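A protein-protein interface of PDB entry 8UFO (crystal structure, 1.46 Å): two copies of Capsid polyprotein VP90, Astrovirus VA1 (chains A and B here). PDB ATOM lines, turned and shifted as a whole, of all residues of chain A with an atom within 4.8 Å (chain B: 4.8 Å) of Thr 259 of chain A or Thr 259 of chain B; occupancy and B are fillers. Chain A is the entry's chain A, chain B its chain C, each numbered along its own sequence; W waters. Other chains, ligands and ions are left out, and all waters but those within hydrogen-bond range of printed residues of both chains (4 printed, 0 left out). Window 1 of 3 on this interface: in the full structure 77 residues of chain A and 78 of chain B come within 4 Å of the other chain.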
ATOM      1  N   VAL A  37       0.078   3.636  -7.982  1.00  0.00           N
ATOM      2  CA  VAL A  37      -1.335   3.969  -7.821  1.00  0.00           C
ATOM      3  C   VAL A  37      -2.262   3.197  -8.742  1.00  0.00           C
ATOM      4  O   VAL A  37      -3.490   3.281  -8.580  1.00  0.00           O
ATOM      5  CB  VAL A  37      -1.644   5.449  -8.124  1.00  0.00           C
ATOM      6  CG1 VAL A  37      -1.118   6.329  -7.041  1.00  0.00           C
ATOM      7  CG2 VAL A  37      -1.186   5.876  -9.537  1.00  0.00           C
ATOM      8  N   ASN A  38      -1.735   2.465  -9.710  1.00  0.00           N
ATOM      9  CA  ASN A  38      -2.560   1.741 -10.666  1.00  0.00           C
ATOM     10  C   ASN A  38      -2.217   0.263 -10.687  1.00  0.00           C
ATOM     11  O   ASN A  38      -2.124  -0.365 -11.745  1.00  0.00           O
ATOM     12  CB  ASN A  38      -2.466   2.346 -12.068  1.00  0.00           C
ATOM     13  CG  ASN A  38      -3.534   3.377 -12.326  1.00  0.00           C
ATOM     14  OD1 ASN A  38      -4.654   3.268 -11.827  1.00  0.00           O
ATOM     15  ND2 ASN A  38      -3.173   4.415 -13.067  1.00  0.00           N
ATOM     16  N   SER A 167      -0.661  -3.000 -14.491  1.00  0.00           N
ATOM     17  CA  SER A 167      -0.535  -1.555 -14.485  1.00  0.00           C
ATOM     18  C   SER A 167      -0.324  -1.044 -15.897  1.00  0.00           C
ATOM     19  O   SER A 167       0.311  -1.715 -16.717  1.00  0.00           O
ATOM     20  CB  SER A 167       0.674  -1.113 -13.653  1.00  0.00           C
ATOM     21  OG  SER A 167       0.763   0.301 -13.617  1.00  0.00           O
ATOM     22  N   PRO A 168      -0.804   0.157 -16.193  1.00  0.00           N
ATOM     23  CA  PRO A 168      -0.456   0.816 -17.455  1.00  0.00           C
ATOM     24  C   PRO A 168       0.958   1.372 -17.417  1.00  0.00           C
ATOM     25  O   PRO A 168       1.509   1.673 -16.357  1.00  0.00           O
ATOM     26  CB  PRO A 168      -1.476   1.959 -17.525  1.00  0.00           C
ATOM     27  CG  PRO A 168      -1.728   2.310 -16.061  1.00  0.00           C
ATOM     28  CD  PRO A 168      -1.719   0.962 -15.361  1.00  0.00           C
ATOM     29  N   TYR A 255      -5.537  10.570 -17.477  1.00  0.00           N
ATOM     30  CA  TYR A 255      -4.189  10.546 -16.903  1.00  0.00           C
ATOM     31  C   TYR A 255      -4.156   9.751 -15.611  1.00  0.00           C
ATOM     32  O   TYR A 255      -3.204   8.995 -15.366  1.00  0.00           O
ATOM     33  CB  TYR A 255      -3.617  11.965 -16.732  1.00  0.00           C
ATOM     34  CG  TYR A 255      -3.661  12.747 -18.030  1.00  0.00           C
ATOM     35  CD1 TYR A 255      -3.086  12.252 -19.193  1.00  0.00           C
ATOM     36  CD2 TYR A 255      -4.333  13.955 -18.104  1.00  0.00           C
ATOM     37  CE1 TYR A 255      -3.179  12.960 -20.405  1.00  0.00           C
ATOM     38  CE2 TYR A 255      -4.427  14.668 -19.305  1.00  0.00           C
ATOM     39  CZ  TYR A 255      -3.849  14.159 -20.446  1.00  0.00           C
ATOM     40  OH  TYR A 255      -3.963  14.862 -21.623  1.00  0.00           O
ATOM     41  N   ARG A 256      -5.208   9.861 -14.799  1.00  0.00           N
ATOM     42  CA  ARG A 256      -5.300   9.026 -13.607  1.00  0.00           C
ATOM     43  C   ARG A 256      -5.360   7.547 -13.973  1.00  0.00           C
ATOM     44  O   ARG A 256      -4.768   6.708 -13.279  1.00  0.00           O
ATOM     45  CB  ARG A 256      -6.528   9.427 -12.780  1.00  0.00           C
ATOM     46  CG  ARG A 256      -6.774   8.503 -11.562  1.00  0.00           C
ATOM     47  CD  ARG A 256      -5.595   8.510 -10.565  1.00  0.00           C
ATOM     48  NE  ARG A 256      -5.796   7.592  -9.442  1.00  0.00           N
ATOM     49  CZ  ARG A 256      -5.534   6.291  -9.505  1.00  0.00           C
ATOM     50  NH1 ARG A 256      -5.114   5.722 -10.629  1.00  0.00           N
ATOM     51  NH2 ARG A 256      -5.734   5.529  -8.427  1.00  0.00           N
ATOM     52  N   ALA A 257      -6.065   7.201 -15.062  1.00  0.00           N
ATOM     53  CA  ALA A 257      -6.178   5.800 -15.462  1.00  0.00           C
ATOM     54  C   ALA A 257      -4.912   5.244 -16.110  1.00  0.00           C
ATOM     55  O   ALA A 257      -4.696   4.023 -16.077  1.00  0.00           O
ATOM     56  CB  ALA A 257      -7.353   5.629 -16.430  1.00  0.00           C
ATOM     57  N   LEU A 258      -4.070   6.095 -16.702  1.00  0.00           N
ATOM     58  CA  LEU A 258      -2.922   5.602 -17.452  1.00  0.00           C
ATOM     59  C   LEU A 258      -1.582   5.782 -16.753  1.00  0.00           C
ATOM     60  O   LEU A 258      -0.582   5.226 -17.234  1.00  0.00           O
ATOM     61  CB  LEU A 258      -2.879   6.245 -18.848  1.00  0.00           C
ATOM     62  CG  LEU A 258      -3.940   5.675 -19.792  1.00  0.00           C
ATOM     63  CD1 LEU A 258      -3.997   6.541 -21.039  1.00  0.00           C
ATOM     64  CD2 LEU A 258      -3.664   4.218 -20.134  1.00  0.00           C
ATOM     65  N   THR A 259      -1.519   6.499 -15.635  1.00  0.00           N
ATOM     66  CA  THR A 259      -0.227   6.731 -15.004  1.00  0.00           C
ATOM     67  C   THR A 259       0.289   5.468 -14.318  1.00  0.00           C
ATOM     68  O   THR A 259      -0.478   4.644 -13.811  1.00  0.00           O
ATOM     69  CB  THR A 259      -0.282   7.893 -14.010  1.00  0.00           C
ATOM     70  OG1 THR A 259       1.064   8.201 -13.620  1.00  0.00           O
ATOM     71  CG2 THR A 259      -1.104   7.547 -12.759  1.00  0.00           C
ATOM     72  N   SER A 260       1.605   5.302 -14.313  1.00  0.00           N
ATOM     73  CA  SER A 260       2.169   4.173 -13.588  1.00  0.00           C
ATOM     74  C   SER A 260       2.446   4.512 -12.137  1.00  0.00           C
ATOM     75  O   SER A 260       2.560   3.601 -11.307  1.00  0.00           O
ATOM     76  CB  SER A 260       3.473   3.689 -14.231  1.00  0.00           C
ATOM     77  OG  SER A 260       3.327   3.430 -15.626  1.00  0.00           O
ATOM     78  N   VAL A 261       2.584   5.802 -11.817  1.00  0.00           N
ATOM     79  CA  VAL A 261       2.979   6.244 -10.488  1.00  0.00           C
ATOM     80  C   VAL A 261       2.215   7.517 -10.148  1.00  0.00           C
ATOM     81  O   VAL A 261       1.805   8.284 -11.022  1.00  0.00           O
ATOM     82  CB  VAL A 261       4.501   6.520 -10.369  1.00  0.00           C
ATOM     83  CG1 VAL A 261       5.306   5.235 -10.241  1.00  0.00           C
ATOM     84  CG2 VAL A 261       5.012   7.378 -11.521  1.00  0.00           C
ATOM     85  N   VAL B  37       2.933  11.560 -23.888  1.00  0.00           N
ATOM     86  CA  VAL B  37       2.405  12.864 -23.496  1.00  0.00           C
ATOM     87  C   VAL B  37       3.345  13.646 -22.584  1.00  0.00           C
ATOM     88  O   VAL B  37       3.114  14.843 -22.360  1.00  0.00           O
ATOM     89  CB  VAL B  37       1.022  12.616 -22.849  1.00  0.00           C
ATOM     90  CG1 VAL B  37       1.171  12.087 -21.427  1.00  0.00           C
ATOM     91  CG2 VAL B  37       0.150  13.852 -22.872  1.00  0.00           C
ATOM     92  N   ASN B  38       4.388  13.018 -22.049  1.00  0.00           N
ATOM     93  CA  ASN B  38       5.296  13.660 -21.103  1.00  0.00           C
ATOM     94  C   ASN B  38       6.736  13.552 -21.567  1.00  0.00           C
ATOM     95  O   ASN B  38       7.646  13.232 -20.796  1.00  0.00           O
ATOM     96  CB  ASN B  38       5.146  13.101 -19.691  1.00  0.00           C
ATOM     97  CG  ASN B  38       4.164  13.897 -18.867  1.00  0.00           C
ATOM     98  OD1 ASN B  38       4.092  15.121 -18.990  1.00  0.00           O
ATOM     99  ND2 ASN B  38       3.391  13.212 -18.026  1.00  0.00           N
ATOM    100  N   PRO B 168       8.534  10.600 -17.015  1.00  0.00           N
ATOM    101  CA  PRO B 168       8.301   9.853 -15.775  1.00  0.00           C
ATOM    102  C   PRO B 168       7.831   8.432 -16.058  1.00  0.00           C
ATOM    103  O   PRO B 168       7.229   8.139 -17.099  1.00  0.00           O
ATOM    104  CB  PRO B 168       7.172  10.652 -15.108  1.00  0.00           C
ATOM    105  CG  PRO B 168       6.377  11.176 -16.274  1.00  0.00           C
ATOM    106  CD  PRO B 168       7.426  11.526 -17.321  1.00  0.00           C
ATOM    107  N   TYR B 255      -1.102  13.600 -11.521  1.00  0.00           N
ATOM    108  CA  TYR B 255      -1.229  12.485 -12.457  1.00  0.00           C
ATOM    109  C   TYR B 255      -0.863  12.906 -13.874  1.00  0.00           C
ATOM    110  O   TYR B 255      -0.166  12.164 -14.582  1.00  0.00           O
ATOM    111  CB  TYR B 255      -2.609  11.817 -12.361  1.00  0.00           C
ATOM    112  CG  TYR B 255      -2.952  11.393 -10.945  1.00  0.00           C
ATOM    113  CD1 TYR B 255      -2.096  10.562 -10.216  1.00  0.00           C
ATOM    114  CD2 TYR B 255      -4.102  11.857 -10.318  1.00  0.00           C
ATOM    115  CE1 TYR B 255      -2.385  10.207  -8.909  1.00  0.00           C
ATOM    116  CE2 TYR B 255      -4.397  11.499  -9.005  1.00  0.00           C
ATOM    117  CZ  TYR B 255      -3.536  10.678  -8.315  1.00  0.00           C
ATOM    118  OH  TYR B 255      -3.816  10.337  -7.013  1.00  0.00           O
ATOM    119  N   ARG B 256      -1.250  14.122 -14.273  1.00  0.00           N
ATOM    120  CA  ARG B 256      -0.825  14.641 -15.570  1.00  0.00           C
ATOM    121  C   ARG B 256       0.694  14.733 -15.646  1.00  0.00           C
ATOM    122  O   ARG B 256       1.278  14.439 -16.692  1.00  0.00           O
ATOM    123  CB  ARG B 256      -1.470  16.009 -15.817  1.00  0.00           C
ATOM    124  CG  ARG B 256      -1.000  16.714 -17.102  1.00  0.00           C
ATOM    125  CD  ARG B 256      -1.315  15.881 -18.357  1.00  0.00           C
ATOM    126  NE  ARG B 256      -0.750  16.487 -19.563  1.00  0.00           N
ATOM    127  CZ  ARG B 256       0.507  16.330 -19.949  1.00  0.00           C
ATOM    128  NH1 ARG B 256       1.376  15.641 -19.216  1.00  0.00           N
ATOM    129  NH2 ARG B 256       0.913  16.895 -21.083  1.00  0.00           N
ATOM    130  N   ALA B 257       1.356  15.114 -14.542  1.00  0.00           N
ATOM    131  CA  ALA B 257       2.806  15.284 -14.577  1.00  0.00           C
ATOM    132  C   ALA B 257       3.567  13.972 -14.502  1.00  0.00           C
ATOM    133  O   ALA B 257       4.734  13.931 -14.919  1.00  0.00           O
ATOM    134  CB  ALA B 257       3.265  16.171 -13.416  1.00  0.00           C
ATOM    135  N   LEU B 258       2.958  12.903 -13.980  1.00  0.00           N
ATOM    136  CA  LEU B 258       3.695  11.675 -13.745  1.00  0.00           C
ATOM    137  C   LEU B 258       3.359  10.548 -14.714  1.00  0.00           C
ATOM    138  O   LEU B 258       4.062   9.533 -14.720  1.00  0.00           O
ATOM    139  CB  LEU B 258       3.501  11.198 -12.298  1.00  0.00           C
ATOM    140  CG  LEU B 258       4.290  12.019 -11.277  1.00  0.00           C
ATOM    141  CD1 LEU B 258       3.887  11.596  -9.863  1.00  0.00           C
ATOM    142  CD2 LEU B 258       5.790  11.783 -11.490  1.00  0.00           C
ATOM    143  N   THR B 259       2.328  10.684 -15.535  1.00  0.00           N
ATOM    144  CA  THR B 259       1.975   9.598 -16.443  1.00  0.00           C
ATOM    145  C   THR B 259       3.004   9.455 -17.570  1.00  0.00           C
ATOM    146  O   THR B 259       3.580  10.431 -18.041  1.00  0.00           O
ATOM    147  CB  THR B 259       0.559   9.782 -17.007  1.00  0.00           C
ATOM    148  OG1 THR B 259       0.225   8.586 -17.717  1.00  0.00           O
ATOM    149  CG2 THR B 259       0.453  11.003 -17.945  1.00  0.00           C
ATOM    150  N   SER B 260       3.234   8.213 -18.002  1.00  0.00           N
ATOM    151  CA  SER B 260       4.126   7.990 -19.133  1.00  0.00           C
ATOM    152  C   SER B 260       3.406   8.095 -20.461  1.00  0.00           C
ATOM    153  O   SER B 260       4.059   8.367 -21.476  1.00  0.00           O
ATOM    154  CB  SER B 260       4.785   6.604 -19.066  1.00  0.00           C
ATOM    155  OG  SER B 260       5.424   6.393 -17.814  1.00  0.00           O
ATOM    156  N   VAL B 261       2.087   7.890 -20.472  1.00  0.00           N
ATOM    157  CA  VAL B 261       1.284   7.837 -21.690  1.00  0.00           C
ATOM    158  C   VAL B 261      -0.063   8.497 -21.422  1.00  0.00           C
ATOM    159  O   VAL B 261      -0.554   8.554 -20.289  1.00  0.00           O
ATOM    160  CB  VAL B 261       1.050   6.392 -22.199  1.00  0.00           C
ATOM    161  CG1 VAL B 261       2.279   5.847 -22.947  1.00  0.00           C
ATOM    162  CG2 VAL B 261       0.627   5.438 -21.068  1.00  0.00           C
HETATM  163  O   HOH W   1      -6.361   9.261  -7.026  1.00  0.00           O
HETATM  164  O   HOH W   2       3.972   6.783 -15.135  1.00  0.00           O
HETATM  165  O   HOH W   3      -3.072  17.493 -21.113  1.00  0.00           O
HETATM  166  O   HOH W   4       2.132   5.504 -17.540  1.00  0.00           O
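The backbone carbonyl oxygen (O) of Leu 258 of chain A lies close to the side-chain hydroxyl (OG1) of Thr 259 of chain B, 3.5 Å away.
The side-chain hydroxyl of Thr 259 of chain A lies within hydrogen-bond range of the backbone carbonyl oxygen of Leu 258 of chain B, 3.5 Å away.
The backbone NH (N) of Thr 259 of chain B lies close to the side-chain hydroxyl (OG1) of Thr 259 of chain A (3.4 Å).
The guanidinium group of Arg 256 of chain A lies within hydrogen-bond range of the backbone carbonyl oxygen of Val 37 of chain A, 3.2 Å away.
The side-chain amide oxygen (OD1) of Asn 38 of chain A lies within hydrogen-bond range of the guanidinium group (NH1) of Arg 256 of chain A.
ND2 of Asn 38 of chain A sits at hydrogen-bond distance from O of Thr 259 of chain A.
The backbone carbonyl oxygen of Val 261 of chain A sits at hydrogen-bond distance from the side-chain hydroxyl of Thr 259 of chain A, 2.7 Å away.
NH2 of Arg 256 of chain B lies within hydrogen-bond range of O of Val 37 of chain B (3.3 Å).
The side-chain hydroxyl (OG1) of Thr 259 of chain B lies within hydrogen-bond range of the backbone carbonyl oxygen (O) of Val 261 of chain B (2.7 Å).
Tyr 255 of chain A touches Arg 256 of chain B (CE2 to CD, 3.5 Å).
Tyr 255 of chain A touches Thr 259 of chain B.
Arg 256 of chain A touches Tyr 255 of chain B.
Val 261 of chain B touches Leu 258 of chain A.
Val 261 of chain A touches Leu 258 of chain B (O to CB, 3.6 Å).
Printed residues of chain B within 4 Å of Tyr 255 of chain A: Arg 256 (3.5 Å) and Thr 259 (3.96 Å).
Of the printed residues of chain B, Arg 256 of chain A touches Tyr 255 (3.6 Å).
Thr 259 of chain A touches just these residues of chain B: Leu 258 (3.5 Å) and Thr 259 (3.3 Å).
Of the printed residues of chain B, Val 261 of chain A touches Leu 258.
Pro 168 of chain B touches none of the printed residues of chain A.
Printed residues of chain A within 4 Å of Arg 256 of chain B: Tyr 255 (3.5 Å).
Of the printed residues of chain A, Leu 258 of chain B touches Thr 259 and Val 261.
Thr 259 of chain B touches three residues of chain A.
The nearest residue of chain B that does not touch Thr 259 of chain A is Tyr 255 of chain B (4.1 Å).
The nearest printed residue of chain A that does not touch Thr 259 of chain B is Ser 260 of chain A (4.8 Å).
The nearest printed residue of chain A that does not touch Val 261 of chain B is Tyr 255 of chain A (4.6 Å).
Printed residues of chain A that touch a printed residue of chain B: Tyr 255, Arg 256, Leu 258, Thr 259 and Val 261.
Hydrophobic or aromatic side chains of chain A that line the printed part of chain B: Tyr 255, Leu 258 and Val 261.
Hydrophobic or aromatic side chains of chain B within 4 Å of the printed part of chain A: Tyr 255 and Leu 258.
Among the printed residues, no Asp or Glu carboxylate lies within 4 Å of a Lys or Arg side-chain nitrogen of the other chain.
Tyr 255 of chain A touches Arg 256 of chain B, and with the chains exchanged Arg 256 of chain A touches Tyr 255 of chain B.
Tyr 255 of chain A touches Thr 259 of chain B, but with the chains exchanged Thr 259 of chain A does not touch Tyr 255 of chain B (4.1 Å).
Leu 258 of chain A touches Val 261 of chain B, and with the chains exchanged Val 261 of chain A touches Leu 258 of chain B.
Thr 259 of chain A touches its own counterpart, Thr 259 of chain B.
10 positions are printed for both chains.
Of the 8 pairs that touch across the chains among the printed residues, 7 have their exchanged pair printed and touching as well.
Water W4 lies within hydrogen-bond range of the backbone carbonyl oxygen (O) of Leu 258 of chain A (2.7 Å), the backbone NH (N) of Ser 260 of chain B (3.0 Å) and the side-chain hydroxyl (OG) of Ser 260 of chain A (3.1 Å).
Water W1 bridges OH of Tyr 255 of chain B and NE of Arg 256 of chain A.
Water W2 lies within hydrogen-bond range of O of Leu 258 of chain B (2.8 Å), N of Ser 260 of chain A (2.9 Å) and OG of Ser 260 of chain B (3.1 Å).
Water W3 lies within hydrogen-bond range of OH of Tyr 255 of chain A (2.8 Å) and NE of Arg 256 of chain B (3.0 Å).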
